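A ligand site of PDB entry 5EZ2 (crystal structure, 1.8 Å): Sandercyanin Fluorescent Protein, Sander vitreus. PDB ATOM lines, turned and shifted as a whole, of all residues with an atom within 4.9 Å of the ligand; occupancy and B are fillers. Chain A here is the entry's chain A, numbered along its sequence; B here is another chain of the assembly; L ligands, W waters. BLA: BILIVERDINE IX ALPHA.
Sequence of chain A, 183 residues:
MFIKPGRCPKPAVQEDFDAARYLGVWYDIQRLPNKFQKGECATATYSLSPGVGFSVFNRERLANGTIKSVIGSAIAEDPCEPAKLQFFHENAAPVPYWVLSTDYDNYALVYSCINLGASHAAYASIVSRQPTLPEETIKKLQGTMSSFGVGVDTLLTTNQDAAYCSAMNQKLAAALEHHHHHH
O2D of the ligand sits close to OE2 of Glu 60 (2.4 Å).
A nitrogen (ND) of the ligand sits at hydrogen-bond distance from the side-chain amide nitrogen of Asn 58 (3.2 Å).
O1D of the ligand lies within salt-bridge range of NZ of Lys 68, 3.6 Å away.
N of Lys 38 lies within hydrogen-bond range of OE2 of Glu 60, 2.8 Å away.
N of Thr 43 is in hydrogen-bond range of O of Arg 59, at 2.9 Å.
O of Pro 96 sits at hydrogen-bond distance from OG of Ser 112 (2.5 Å).
The side-chain hydroxyl (OH) of Tyr 123 lies within hydrogen-bond range of the side-chain amide oxygen (OE1) of Gln 37, at 3.3 Å.
The backbone NH (N) of Asp 28 lies within hydrogen-bond range of the backbone carbonyl oxygen (O) of Ala 42, at 3.0 Å.
N of Val 110 lies within hydrogen-bond range of O of Ser 125, at 2.9 Å.
The side-chain hydroxyl of Tyr 97 lies within hydrogen-bond range of the side-chain hydroxyl of Tyr 46 (2.7 Å).
The backbone carbonyl oxygen (O) of Ala 44 lies within hydrogen-bond range of the backbone NH (N) of Trp 26 (2.8 Å).
O of Leu 116 of chain B lies close to OB of the ligand.
Residues that only touch the ligand: Phe 36, Ala 118 of chain B, Arg 59, His 89, Ser 112, Val 127, Gly 117 of chain B, Tyr 123, Val 70, Asp 28, Ala 92, Val 95, Ile 114, Val 110, Tyr 97, Ser 125 and Ala 44.
Hydrophobic or aromatic side chains within 4 Å of the ligand: Phe 36, Ala 44, Val 70, His 89, Ala 92, Val 95, Tyr 97, Val 110, Ile 114, Tyr 123, Val 127 and Ala 118 of chain B.
Within 4 Å of the ligand: Asp 28, Phe 36, Ala 44, Asn 58, Arg 59, Glu 60, Lys 68, Val 70, His 89, Ala 92, Val 95, Tyr 97, Val 110, Ser 112, Ile 114, Tyr 123, Ser 125, Val 127, Leu 116 of chain B, Gly 117 of chain B and Ala 118 of chain B.
Water W1 lies within hydrogen-bond range of O1A of the ligand, NZ of Lys 38, O of Phe 36 and NZ of Lys 68.
Water W2 lies within hydrogen-bond range of NE2 of His 89 (2.7 Å), OC of the ligand (2.9 Å) and ND2 of Asn 58 (3.0 Å).
Water W5 lies within hydrogen-bond range of the backbone NH (N) of Ala 118 of chain B (2.9 Å), an oxygen (O2A) of the ligand (3.0 Å) and the backbone carbonyl oxygen (O) of Leu 116 of chain B (3.5 Å).
Water W3 lies within hydrogen-bond range of the backbone carbonyl oxygen of Leu 116 of chain B (2.9 Å) and an oxygen (OB) of the ligand (3.0 Å).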
ATOM      1  N   TRP A  26     -14.993   2.912  25.606  1.00  0.00           N
ATOM      2  CA  TRP A  26     -13.912   2.203  24.930  1.00  0.00           C
ATOM      3  C   TRP A  26     -14.413   1.589  23.631  1.00  0.00           C
ATOM      4  O   TRP A  26     -15.533   1.059  23.578  1.00  0.00           O
ATOM      5  CB  TRP A  26     -13.376   1.075  25.829  1.00  0.00           C
ATOM      6  CG  TRP A  26     -12.646   1.560  27.049  1.00  0.00           C
ATOM      7  CD1 TRP A  26     -13.157   1.719  28.303  1.00  0.00           C
ATOM      8  CD2 TRP A  26     -11.262   1.925  27.127  1.00  0.00           C
ATOM      9  NE1 TRP A  26     -12.176   2.163  29.162  1.00  0.00           N
ATOM     10  CE2 TRP A  26     -10.999   2.289  28.468  1.00  0.00           C
ATOM     11  CE3 TRP A  26     -10.221   1.966  26.202  1.00  0.00           C
ATOM     12  CZ2 TRP A  26      -9.734   2.704  28.890  1.00  0.00           C
ATOM     13  CZ3 TRP A  26      -8.967   2.382  26.624  1.00  0.00           C
ATOM     14  CH2 TRP A  26      -8.733   2.750  27.950  1.00  0.00           C
ATOM     15  N   TYR A  27     -13.591   1.642  22.581  1.00  0.00           N
ATOM     16  CA  TYR A  27     -13.923   1.009  21.299  1.00  0.00           C
ATOM     17  C   TYR A  27     -13.181  -0.295  21.148  1.00  0.00           C
ATOM     18  O   TYR A  27     -11.965  -0.366  21.402  1.00  0.00           O
ATOM     19  CB  TYR A  27     -13.552   1.935  20.123  1.00  0.00           C
ATOM     20  CG  TYR A  27     -14.335   3.208  20.121  1.00  0.00           C
ATOM     21  CD1 TYR A  27     -13.928   4.307  20.874  1.00  0.00           C
ATOM     22  CD2 TYR A  27     -15.501   3.322  19.375  1.00  0.00           C
ATOM     23  CE1 TYR A  27     -14.652   5.474  20.877  1.00  0.00           C
ATOM     24  CE2 TYR A  27     -16.224   4.489  19.364  1.00  0.00           C
ATOM     25  CZ  TYR A  27     -15.800   5.565  20.122  1.00  0.00           C
ATOM     26  OH  TYR A  27     -16.545   6.719  20.124  1.00  0.00           O
ATOM     27  N   ASP A  28     -13.887  -1.337  20.707  1.00  0.00           N
ATOM     28  CA  ASP A  28     -13.251  -2.602  20.415  1.00  0.00           C
ATOM     29  C   ASP A  28     -12.430  -2.490  19.136  1.00  0.00           C
ATOM     30  O   ASP A  28     -12.961  -2.104  18.082  1.00  0.00           O
ATOM     31  CB  ASP A  28     -14.289  -3.716  20.265  1.00  0.00           C
ATOM     32  CG  ASP A  28     -13.657  -5.096  20.197  1.00  0.00           C
ATOM     33  OD1 ASP A  28     -13.145  -5.563  21.230  1.00  0.00           O
ATOM     34  OD2 ASP A  28     -13.679  -5.718  19.129  1.00  0.00           O
ATOM     35  N   LYS A  35     -18.548 -15.877  21.431  1.00  0.00           N
ATOM     36  CA  LYS A  35     -19.946 -16.199  21.150  1.00  0.00           C
ATOM     37  C   LYS A  35     -20.870 -15.007  21.314  1.00  0.00           C
ATOM     38  O   LYS A  35     -21.979 -14.998  20.780  1.00  0.00           O
ATOM     39  CB  LYS A  35     -20.417 -17.345  22.046  1.00  0.00           C
ATOM     40  CG  LYS A  35     -19.694 -18.645  21.803  1.00  0.00           C
ATOM     41  CD  LYS A  35     -20.024 -19.177  20.424  1.00  0.00           C
ATOM     42  CE  LYS A  35     -19.536 -20.601  20.235  1.00  0.00           C
ATOM     43  NZ  LYS A  35     -20.065 -21.098  18.933  1.00  0.00           N
ATOM     44  N   PHE A  36     -20.430 -13.980  22.047  1.00  0.00           N
ATOM     45  CA  PHE A  36     -21.349 -12.907  22.399  1.00  0.00           C
ATOM     46  C   PHE A  36     -21.398 -11.754  21.393  1.00  0.00           C
ATOM     47  O   PHE A  36     -22.449 -11.143  21.215  1.00  0.00           O
ATOM     48  CB  PHE A  36     -21.099 -12.377  23.812  1.00  0.00           C
ATOM     49  CG  PHE A  36     -19.660 -12.040  24.117  1.00  0.00           C
ATOM     50  CD1 PHE A  36     -18.800 -13.003  24.598  1.00  0.00           C
ATOM     51  CD2 PHE A  36     -19.192 -10.737  23.960  1.00  0.00           C
ATOM     52  CE1 PHE A  36     -17.485 -12.696  24.897  1.00  0.00           C
ATOM     53  CE2 PHE A  36     -17.876 -10.423  24.267  1.00  0.00           C
ATOM     54  CZ  PHE A  36     -17.029 -11.412  24.731  1.00  0.00           C
ATOM     55  N   GLN A  37     -20.274 -11.455  20.742  1.00  0.00           N
ATOM     56  CA  GLN A  37     -20.252 -10.382  19.744  1.00  0.00           C
ATOM     57  C   GLN A  37     -20.712 -10.903  18.391  1.00  0.00           C
ATOM     58  O   GLN A  37     -20.035 -11.717  17.752  1.00  0.00           O
ATOM     59  CB  GLN A  37     -18.869  -9.762  19.626  1.00  0.00           C
ATOM     60  CG  GLN A  37     -18.536  -8.747  20.725  1.00  0.00           C
ATOM     61  CD  GLN A  37     -17.106  -8.254  20.618  1.00  0.00           C
ATOM     62  OE1 GLN A  37     -16.243  -8.674  21.378  1.00  0.00           O
ATOM     63  NE2 GLN A  37     -16.854  -7.385  19.640  1.00  0.00           N
ATOM     64  N   LYS A  38     -21.865 -10.435  17.949  1.00  0.00           N
ATOM     65  CA  LYS A  38     -22.476 -10.938  16.723  1.00  0.00           C
ATOM     66  C   LYS A  38     -22.429  -9.932  15.583  1.00  0.00           C
ATOM     67  O   LYS A  38     -22.879 -10.228  14.472  1.00  0.00           O
ATOM     68  CB  LYS A  38     -23.904 -11.393  17.032  1.00  0.00           C
ATOM     69  CG  LYS A  38     -23.915 -12.672  17.848  1.00  0.00           C
ATOM     70  CD  LYS A  38     -25.097 -12.720  18.777  1.00  0.00           C
ATOM     71  CE  LYS A  38     -25.013 -13.944  19.671  1.00  0.00           C
ATOM     72  NZ  LYS A  38     -25.938 -13.813  20.836  1.00  0.00           N
ATOM     73  N   ALA A  42     -18.380  -2.498  17.999  1.00  0.00           N
ATOM     74  CA  ALA A  42     -18.590  -2.717  19.437  1.00  0.00           C
ATOM     75  C   ALA A  42     -17.966  -1.637  20.306  1.00  0.00           C
ATOM     76  O   ALA A  42     -16.832  -1.203  20.088  1.00  0.00           O
ATOM     77  CB  ALA A  42     -18.083  -4.081  19.858  1.00  0.00           C
ATOM     78  N   THR A  43     -18.720  -1.231  21.323  1.00  0.00           N
ATOM     79  CA  THR A  43     -18.203  -0.308  22.303  1.00  0.00           C
ATOM     80  C   THR A  43     -18.600  -0.775  23.700  1.00  0.00           C
ATOM     81  O   THR A  43     -19.653  -1.413  23.886  1.00  0.00           O
ATOM     82  CB  THR A  43     -18.717   1.106  22.036  1.00  0.00           C
ATOM     83  OG1 THR A  43     -17.915   2.046  22.761  1.00  0.00           O
ATOM     84  CG2 THR A  43     -20.176   1.237  22.451  1.00  0.00           C
ATOM     85  N   ALA A  44     -17.745  -0.472  24.685  1.00  0.00           N
ATOM     86  CA  ALA A  44     -18.065  -0.683  26.086  1.00  0.00           C
ATOM     87  C   ALA A  44     -18.076   0.653  26.817  1.00  0.00           C
ATOM     88  O   ALA A  44     -17.129   1.439  26.699  1.00  0.00           O
ATOM     89  CB  ALA A  44     -17.044  -1.628  26.721  1.00  0.00           C
ATOM     90  N   TYR A  46     -18.305   2.271  30.611  1.00  0.00           N
ATOM     91  CA  TYR A  46     -18.240   1.990  32.028  1.00  0.00           C
ATOM     92  C   TYR A  46     -18.579   3.272  32.789  1.00  0.00           C
ATOM     93  O   TYR A  46     -18.022   4.344  32.491  1.00  0.00           O
ATOM     94  CB  TYR A  46     -16.839   1.476  32.385  1.00  0.00           C
ATOM     95  CG  TYR A  46     -16.424   0.248  31.588  1.00  0.00           C
ATOM     96  CD1 TYR A  46     -17.297  -0.823  31.403  1.00  0.00           C
ATOM     97  CD2 TYR A  46     -15.179   0.170  31.004  1.00  0.00           C
ATOM     98  CE1 TYR A  46     -16.922  -1.942  30.687  1.00  0.00           C
ATOM     99  CE2 TYR A  46     -14.784  -0.949  30.273  1.00  0.00           C
ATOM    100  CZ  TYR A  46     -15.665  -2.000  30.111  1.00  0.00           C
ATOM    101  OH  TYR A  46     -15.288  -3.103  29.382  1.00  0.00           O
ATOM    102  N   ASN A  58     -22.634  -2.361  27.071  1.00  0.00           N
ATOM    103  CA  ASN A  58     -21.945  -2.740  25.842  1.00  0.00           C
ATOM    104  C   ASN A  58     -22.928  -2.655  24.678  1.00  0.00           C
ATOM    105  O   ASN A  58     -24.078  -3.066  24.827  1.00  0.00           O
ATOM    106  CB  ASN A  58     -21.441  -4.172  25.929  1.00  0.00           C
ATOM    107  CG  ASN A  58     -20.388  -4.371  27.013  1.00  0.00           C
ATOM    108  OD1 ASN A  58     -19.742  -3.422  27.444  1.00  0.00           O
ATOM    109  ND2 ASN A  58     -20.241  -5.616  27.466  1.00  0.00           N
ATOM    110  N   ARG A  59     -22.488  -2.125  23.537  1.00  0.00           N
ATOM    111  CA  ARG A  59     -23.354  -1.985  22.359  1.00  0.00           C
ATOM    112  C   ARG A  59     -22.609  -2.404  21.106  1.00  0.00           C
ATOM    113  O   ARG A  59     -21.399  -2.195  20.989  1.00  0.00           O
ATOM    114  CB  ARG A  59     -23.784  -0.529  22.155  1.00  0.00           C
ATOM    115  CG  ARG A  59     -24.327   0.188  23.355  1.00  0.00           C
ATOM    116  CD  ARG A  59     -24.350   1.682  23.078  1.00  0.00           C
ATOM    117  NE  ARG A  59     -25.446   2.073  22.189  1.00  0.00           N
ATOM    118  CZ  ARG A  59     -25.317   2.909  21.170  1.00  0.00           C
ATOM    119  NH1 ARG A  59     -24.134   3.431  20.876  1.00  0.00           N
ATOM    120  NH2 ARG A  59     -26.372   3.218  20.424  1.00  0.00           N
ATOM    121  N   GLU A  60     -23.341  -2.979  20.155  1.00  0.00           N
ATOM    122  CA  GLU A  60     -22.732  -3.263  18.841  1.00  0.00           C
ATOM    123  C   GLU A  60     -23.780  -3.127  17.744  1.00  0.00           C
ATOM    124  O   GLU A  60     -24.980  -3.032  18.026  1.00  0.00           O
ATOM    125  CB  GLU A  60     -22.091  -4.652  18.793  1.00  0.00           C
ATOM    126  CG  GLU A  60     -23.087  -5.804  18.982  1.00  0.00           C
ATOM    127  CD  GLU A  60     -22.471  -7.170  18.723  1.00  0.00           C
ATOM    128  OE1 GLU A  60     -21.325  -7.225  18.231  1.00  0.00           O
ATOM    129  OE2 GLU A  60     -23.133  -8.194  19.002  1.00  0.00           O
ATOM    130  N   LEU A  62     -25.441  -4.861  14.559  1.00  0.00           N
ATOM    131  CA  LEU A  62     -25.604  -6.124  13.846  1.00  0.00           C
ATOM    132  C   LEU A  62     -25.591  -5.878  12.335  1.00  0.00           C
ATOM    133  O   LEU A  62     -25.760  -4.746  11.885  1.00  0.00           O
ATOM    134  CB  LEU A  62     -26.924  -6.792  14.244  1.00  0.00           C
ATOM    135  CG  LEU A  62     -27.066  -7.123  15.744  1.00  0.00           C
ATOM    136  CD1 LEU A  62     -28.437  -7.706  16.049  1.00  0.00           C
ATOM    137  CD2 LEU A  62     -25.996  -8.100  16.143  1.00  0.00           C
ATOM    138  N   LYS A  68     -27.621  -3.650  19.153  1.00  0.00           N
ATOM    139  CA  LYS A  68     -27.951  -4.578  20.237  1.00  0.00           C
ATOM    140  C   LYS A  68     -27.071  -4.199  21.429  1.00  0.00           C
ATOM    141  O   LYS A  68     -25.922  -3.800  21.250  1.00  0.00           O
ATOM    142  CB  LYS A  68     -27.714  -6.029  19.777  1.00  0.00           C
ATOM    143  CG  LYS A  68     -28.604  -7.069  20.462  1.00  0.00           C
ATOM    144  CD  LYS A  68     -28.302  -8.486  19.957  1.00  0.00           C
ATOM    145  CE  LYS A  68     -28.584  -9.528  21.052  1.00  0.00           C
ATOM    146  NZ  LYS A  68     -27.859 -10.813  20.796  1.00  0.00           N
ATOM    147  N   SER A  69     -27.607  -4.277  22.646  1.00  0.00           N
ATOM    148  CA  SER A  69     -26.814  -3.872  23.810  1.00  0.00           C
ATOM    149  C   SER A  69     -27.102  -4.767  25.019  1.00  0.00           C
ATOM    150  O   SER A  69     -28.093  -5.502  25.020  1.00  0.00           O
ATOM    151  CB  SER A  69     -27.090  -2.414  24.163  1.00  0.00           C
ATOM    152  OG  SER A  69     -28.451  -2.219  24.543  1.00  0.00           O
ATOM    153  N   VAL A  70     -26.221  -4.697  26.011  1.00  0.00           N
ATOM    154  CA  VAL A  70     -26.422  -5.428  27.272  1.00  0.00           C
ATOM    155  C   VAL A  70     -25.934  -4.562  28.431  1.00  0.00           C
ATOM    156  O   VAL A  70     -25.024  -3.753  28.258  1.00  0.00           O
ATOM    157  CB  VAL A  70     -25.710  -6.802  27.285  1.00  0.00           C
ATOM    158  CG1 VAL A  70     -24.204  -6.630  27.241  1.00  0.00           C
ATOM    159  CG2 VAL A  70     -26.078  -7.586  28.538  1.00  0.00           C
ATOM    160  N   HIS A  89     -23.272  -9.815  33.658  1.00  0.00           N
ATOM    161  CA  HIS A  89     -24.096  -9.261  32.577  1.00  0.00           C
ATOM    162  C   HIS A  89     -25.511  -9.797  32.744  1.00  0.00           C
ATOM    163  O   HIS A  89     -25.702 -10.899  33.260  1.00  0.00           O
ATOM    164  CB  HIS A  89     -23.563  -9.703  31.204  1.00  0.00           C
ATOM    165  CG  HIS A  89     -22.168  -9.280  30.898  1.00  0.00           C
ATOM    166  ND1 HIS A  89     -21.052 -10.005  31.293  1.00  0.00           N
ATOM    167  CD2 HIS A  89     -21.688  -8.211  30.193  1.00  0.00           C
ATOM    168  CE1 HIS A  89     -19.968  -9.395  30.856  1.00  0.00           C
ATOM    169  NE2 HIS A  89     -20.311  -8.316  30.191  1.00  0.00           N
ATOM    170  N   ALA A  92     -26.541 -13.583  32.298  1.00  0.00           N
ATOM    171  CA  ALA A  92     -25.365 -14.393  32.047  1.00  0.00           C
ATOM    172  C   ALA A  92     -24.795 -14.846  33.387  1.00  0.00           C
ATOM    173  O   ALA A  92     -25.011 -14.195  34.411  1.00  0.00           O
ATOM    174  CB  ALA A  92     -24.348 -13.592  31.264  1.00  0.00           C
ATOM    175  N   VAL A  95     -18.517 -13.784  34.725  1.00  0.00           N
ATOM    176  CA  VAL A  95     -17.294 -14.094  33.983  1.00  0.00           C
ATOM    177  C   VAL A  95     -16.163 -13.216  34.489  1.00  0.00           C
ATOM    178  O   VAL A  95     -16.383 -12.086  34.925  1.00  0.00           O
ATOM    179  CB  VAL A  95     -17.452 -13.857  32.453  1.00  0.00           C
ATOM    180  CG1 VAL A  95     -18.508 -14.798  31.865  1.00  0.00           C
ATOM    181  CG2 VAL A  95     -17.790 -12.393  32.145  1.00  0.00           C
ATOM    182  N   PRO A  96     -14.931 -13.751  34.436  1.00  0.00           N
ATOM    183  CA  PRO A  96     -13.769 -12.967  34.834  1.00  0.00           C
ATOM    184  C   PRO A  96     -13.448 -11.930  33.753  1.00  0.00           C
ATOM    185  O   PRO A  96     -13.756 -12.133  32.569  1.00  0.00           O
ATOM    186  CB  PRO A  96     -12.662 -14.010  35.000  1.00  0.00           C
ATOM    187  CG  PRO A  96     -13.062 -15.160  34.107  1.00  0.00           C
ATOM    188  CD  PRO A  96     -14.583 -15.103  33.938  1.00  0.00           C
ATOM    189  N   TYR A  97     -12.846 -10.826  34.177  1.00  0.00           N
ATOM    190  CA  TYR A  97     -12.421  -9.741  33.295  1.00  0.00           C
ATOM    191  C   TYR A  97     -11.182  -9.152  33.939  1.00  0.00           C
ATOM    192  O   TYR A  97     -11.261  -8.534  35.005  1.00  0.00           O
ATOM    193  CB  TYR A  97     -13.529  -8.694  33.243  1.00  0.00           C
ATOM    194  CG  TYR A  97     -13.310  -7.454  32.378  1.00  0.00           C
ATOM    195  CD1 TYR A  97     -12.523  -6.406  32.822  1.00  0.00           C
ATOM    196  CD2 TYR A  97     -13.964  -7.311  31.156  1.00  0.00           C
ATOM    197  CE1 TYR A  97     -12.362  -5.234  32.056  1.00  0.00           C
ATOM    198  CE2 TYR A  97     -13.816  -6.158  30.380  1.00  0.00           C
ATOM    199  CZ  TYR A  97     -13.001  -5.129  30.837  1.00  0.00           C
ATOM    200  OH  TYR A  97     -12.842  -3.972  30.084  1.00  0.00           O
ATOM    201  N   VAL A 110      -7.705  -6.397  27.591  1.00  0.00           N
ATOM    202  CA  VAL A 110      -8.498  -7.146  28.561  1.00  0.00           C
ATOM    203  C   VAL A 110      -8.398  -8.643  28.278  1.00  0.00           C
ATOM    204  O   VAL A 110      -8.277  -9.056  27.119  1.00  0.00           O
ATOM    205  CB  VAL A 110      -9.976  -6.656  28.604  1.00  0.00           C
ATOM    206  CG1 VAL A 110     -10.037  -5.168  28.929  1.00  0.00           C
ATOM    207  CG2 VAL A 110     -10.640  -6.910  27.294  1.00  0.00           C
ATOM    208  N   SER A 112      -9.882 -12.727  29.612  1.00  0.00           N
ATOM    209  CA  SER A 112     -10.808 -13.523  30.397  1.00  0.00           C
ATOM    210  C   SER A 112     -10.604 -14.986  30.028  1.00  0.00           C
ATOM    211  O   SER A 112     -10.413 -15.320  28.863  1.00  0.00           O
ATOM    212  CB  SER A 112     -12.250 -13.108  30.072  1.00  0.00           C
ATOM    213  OG  SER A 112     -13.189 -13.838  30.856  1.00  0.00           O
ATOM    214  N   ILE A 114     -11.849 -19.211  31.162  1.00  0.00           N
ATOM    215  CA  ILE A 114     -12.570 -20.162  32.007  1.00  0.00           C
ATOM    216  C   ILE A 114     -12.080 -21.576  31.706  1.00  0.00           C
ATOM    217  O   ILE A 114     -11.955 -21.966  30.527  1.00  0.00           O
ATOM    218  CB  ILE A 114     -14.105 -20.055  31.786  1.00  0.00           C
ATOM    219  CG1 ILE A 114     -14.606 -18.715  32.343  1.00  0.00           C
ATOM    220  CG2 ILE A 114     -14.827 -21.219  32.469  1.00  0.00           C
ATOM    221  CD1 ILE A 114     -16.033 -18.361  31.962  1.00  0.00           C
ATOM    222  N   ALA A 121     -11.439 -21.963  27.676  1.00  0.00           N
ATOM    223  CA  ALA A 121     -12.054 -21.017  26.751  1.00  0.00           C
ATOM    224  C   ALA A 121     -11.623 -19.621  27.142  1.00  0.00           C
ATOM    225  O   ALA A 121     -11.928 -19.140  28.247  1.00  0.00           O
ATOM    226  CB  ALA A 121     -13.574 -21.125  26.821  1.00  0.00           C
ATOM    227  N   TYR A 123     -11.058 -15.338  26.205  1.00  0.00           N
ATOM    228  CA  TYR A 123     -11.429 -14.155  25.443  1.00  0.00           C
ATOM    229  C   TYR A 123     -10.385 -13.072  25.696  1.00  0.00           C
ATOM    230  O   TYR A 123      -9.788 -13.011  26.781  1.00  0.00           O
ATOM    231  CB  TYR A 123     -12.822 -13.676  25.878  1.00  0.00           C
ATOM    232  CG  TYR A 123     -13.166 -12.302  25.333  1.00  0.00           C
ATOM    233  CD1 TYR A 123     -13.464 -12.119  23.987  1.00  0.00           C
ATOM    234  CD2 TYR A 123     -13.162 -11.198  26.163  1.00  0.00           C
ATOM    235  CE1 TYR A 123     -13.752 -10.878  23.495  1.00  0.00           C
ATOM    236  CE2 TYR A 123     -13.469  -9.947  25.665  1.00  0.00           C
ATOM    237  CZ  TYR A 123     -13.760  -9.795  24.344  1.00  0.00           C
ATOM    238  OH  TYR A 123     -14.067  -8.544  23.846  1.00  0.00           O
ATOM    239  N   SER A 125      -9.352  -8.781  24.330  1.00  0.00           N
ATOM    240  CA  SER A 125      -9.727  -7.642  23.514  1.00  0.00           C
ATOM    241  C   SER A 125      -8.699  -6.533  23.656  1.00  0.00           C
ATOM    242  O   SER A 125      -8.183  -6.284  24.735  1.00  0.00           O
ATOM    243  CB  SER A 125     -11.085  -7.113  23.982  1.00  0.00           C
ATOM    244  OG  SER A 125     -11.473  -5.992  23.221  1.00  0.00           O
ATOM    245  N   VAL A 127      -8.826  -2.567  23.249  1.00  0.00           N
ATOM    246  CA  VAL A 127      -9.768  -1.479  23.112  1.00  0.00           C
ATOM    247  C   VAL A 127      -9.036  -0.140  23.114  1.00  0.00           C
ATOM    248  O   VAL A 127      -7.886  -0.050  23.552  1.00  0.00           O
ATOM    249  CB  VAL A 127     -10.827  -1.487  24.233  1.00  0.00           C
ATOM    250  CG1 VAL A 127     -11.681  -2.747  24.137  1.00  0.00           C
ATOM    251  CG2 VAL A 127     -10.170  -1.389  25.620  1.00  0.00           C
ATOM    252  N   LEU B 116     -20.347 -20.471  30.524  1.00  0.00           N
ATOM    253  CA  LEU B 116     -19.470 -19.558  29.828  1.00  0.00           C
ATOM    254  C   LEU B 116     -20.272 -18.308  29.496  1.00  0.00           C
ATOM    255  O   LEU B 116     -20.719 -18.101  28.362  1.00  0.00           O
ATOM    256  CB  LEU B 116     -18.917 -20.195  28.535  1.00  0.00           C
ATOM    257  CG  LEU B 116     -18.151 -21.509  28.754  1.00  0.00           C
ATOM    258  CD1 LEU B 116     -17.886 -22.207  27.428  1.00  0.00           C
ATOM    259  CD2 LEU B 116     -16.832 -21.218  29.442  1.00  0.00           C
ATOM    260  N   GLY B 117     -20.478 -17.465  30.517  1.00  0.00           N
ATOM    261  CA  GLY B 117     -21.256 -16.261  30.338  1.00  0.00           C
ATOM    262  C   GLY B 117     -22.715 -16.597  30.047  1.00  0.00           C
ATOM    263  O   GLY B 117     -23.407 -17.160  30.909  1.00  0.00           O
ATOM    264  N   ALA B 118     -23.169 -16.262  28.847  1.00  0.00           N
ATOM    265  CA  ALA B 118     -24.560 -16.535  28.485  1.00  0.00           C
ATOM    266  C   ALA B 118     -24.646 -17.840  27.684  1.00  0.00           C
ATOM    267  O   ALA B 118     -25.711 -18.188  27.166  1.00  0.00           O
ATOM    268  CB  ALA B 118     -25.155 -15.375  27.695  1.00  0.00           C
HETATM  269  CHA BLA L   1     -22.056  -8.986  25.635  1.00  0.00           C
HETATM  270  NA  BLA L   1     -20.116  -9.919  26.867  1.00  0.00           N
HETATM  271  C1A BLA L   1     -21.445  -9.868  26.637  1.00  0.00           C
HETATM  272  C2A BLA L   1     -22.231 -10.866  27.370  1.00  0.00           C
HETATM  273  C3A BLA L   1     -21.227 -11.564  28.207  1.00  0.00           C
HETATM  274  C4A BLA L   1     -19.954 -10.870  27.803  1.00  0.00           C
HETATM  275  CMA BLA L   1     -21.453 -12.662  29.227  1.00  0.00           C
HETATM  276  CAA BLA L   1     -23.734 -11.017  27.281  1.00  0.00           C
HETATM  277  CBA BLA L   1     -24.180 -12.439  27.093  1.00  0.00           C
HETATM  278  CGA BLA L   1     -24.155 -12.655  25.624  1.00  0.00           C
HETATM  279  O1A BLA L   1     -24.773 -11.809  24.924  1.00  0.00           O
HETATM  280  O2A BLA L   1     -23.539 -13.648  25.202  1.00  0.00           O
HETATM  281  CHB BLA L   1     -18.594 -11.273  28.241  1.00  0.00           C
HETATM  282  NB  BLA L   1     -18.881 -13.783  27.989  1.00  0.00           N
HETATM  283  C1B BLA L   1     -18.125 -12.680  28.196  1.00  0.00           C
HETATM  284  C2B BLA L   1     -16.703 -12.980  28.532  1.00  0.00           C
HETATM  285  C3B BLA L   1     -16.653 -14.446  28.500  1.00  0.00           C
HETATM  286  C4B BLA L   1     -18.036 -14.835  28.156  1.00  0.00           C
HETATM  287  CMB BLA L   1     -15.627 -11.982  28.813  1.00  0.00           C
HETATM  288  OB  BLA L   1     -18.403 -16.063  28.024  1.00  0.00           O
HETATM  289  CAB BLA L   1     -15.455 -15.280  28.759  1.00  0.00           C
HETATM  290  CBB BLA L   1     -15.481 -16.600  28.703  1.00  0.00           C
HETATM  291  NC  BLA L   1     -17.400  -7.012  25.838  1.00  0.00           N
HETATM  292  C1C BLA L   1     -16.184  -6.855  26.398  1.00  0.00           C
HETATM  293  C2C BLA L   1     -15.296  -5.824  25.798  1.00  0.00           C
HETATM  294  C3C BLA L   1     -16.181  -5.362  24.707  1.00  0.00           C
HETATM  295  C4C BLA L   1     -17.426  -6.112  24.843  1.00  0.00           C
HETATM  296  CMC BLA L   1     -13.910  -5.404  26.194  1.00  0.00           C
HETATM  297  OC  BLA L   1     -15.837  -7.568  27.410  1.00  0.00           O
HETATM  298  CAC BLA L   1     -16.037  -4.280  23.705  1.00  0.00           C
HETATM  299  CBC BLA L   1     -15.062  -3.396  23.803  1.00  0.00           C
HETATM  300  CHD BLA L   1     -18.568  -5.977  23.922  1.00  0.00           C
HETATM  301  ND  BLA L   1     -20.071  -7.650  25.002  1.00  0.00           N
HETATM  302  C1D BLA L   1     -19.850  -6.688  24.068  1.00  0.00           C
HETATM  303  C2D BLA L   1     -21.041  -6.236  23.319  1.00  0.00           C
HETATM  304  C3D BLA L   1     -22.102  -7.107  23.838  1.00  0.00           C
HETATM  305  C4D BLA L   1     -21.385  -7.935  24.840  1.00  0.00           C
HETATM  306  CMD BLA L   1     -21.119  -5.168  22.253  1.00  0.00           C
HETATM  307  CAD BLA L   1     -23.543  -7.182  23.409  1.00  0.00           C
HETATM  308  CBD BLA L   1     -23.544  -8.193  22.282  1.00  0.00           C
HETATM  309  CGD BLA L   1     -24.936  -8.308  21.702  1.00  0.00           C
HETATM  310  O1D BLA L   1     -25.901  -8.308  22.498  1.00  0.00           O
HETATM  311  O2D BLA L   1     -25.083  -8.407  20.460  1.00  0.00           O
HETATM  312  O   HOH W   1     -24.899 -11.755  22.376  1.00  0.00           O
HETATM  313  O   HOH W   2     -18.181  -7.106  29.017  1.00  0.00           O
HETATM  314  O   HOH W   3     -20.009 -17.069  25.740  1.00  0.00           O
HETATM  315  O   HOH W   4     -26.136  -9.724  24.958  1.00  0.00           O
HETATM  316  O   HOH W   5     -21.514 -15.077  26.821  1.00  0.00           O
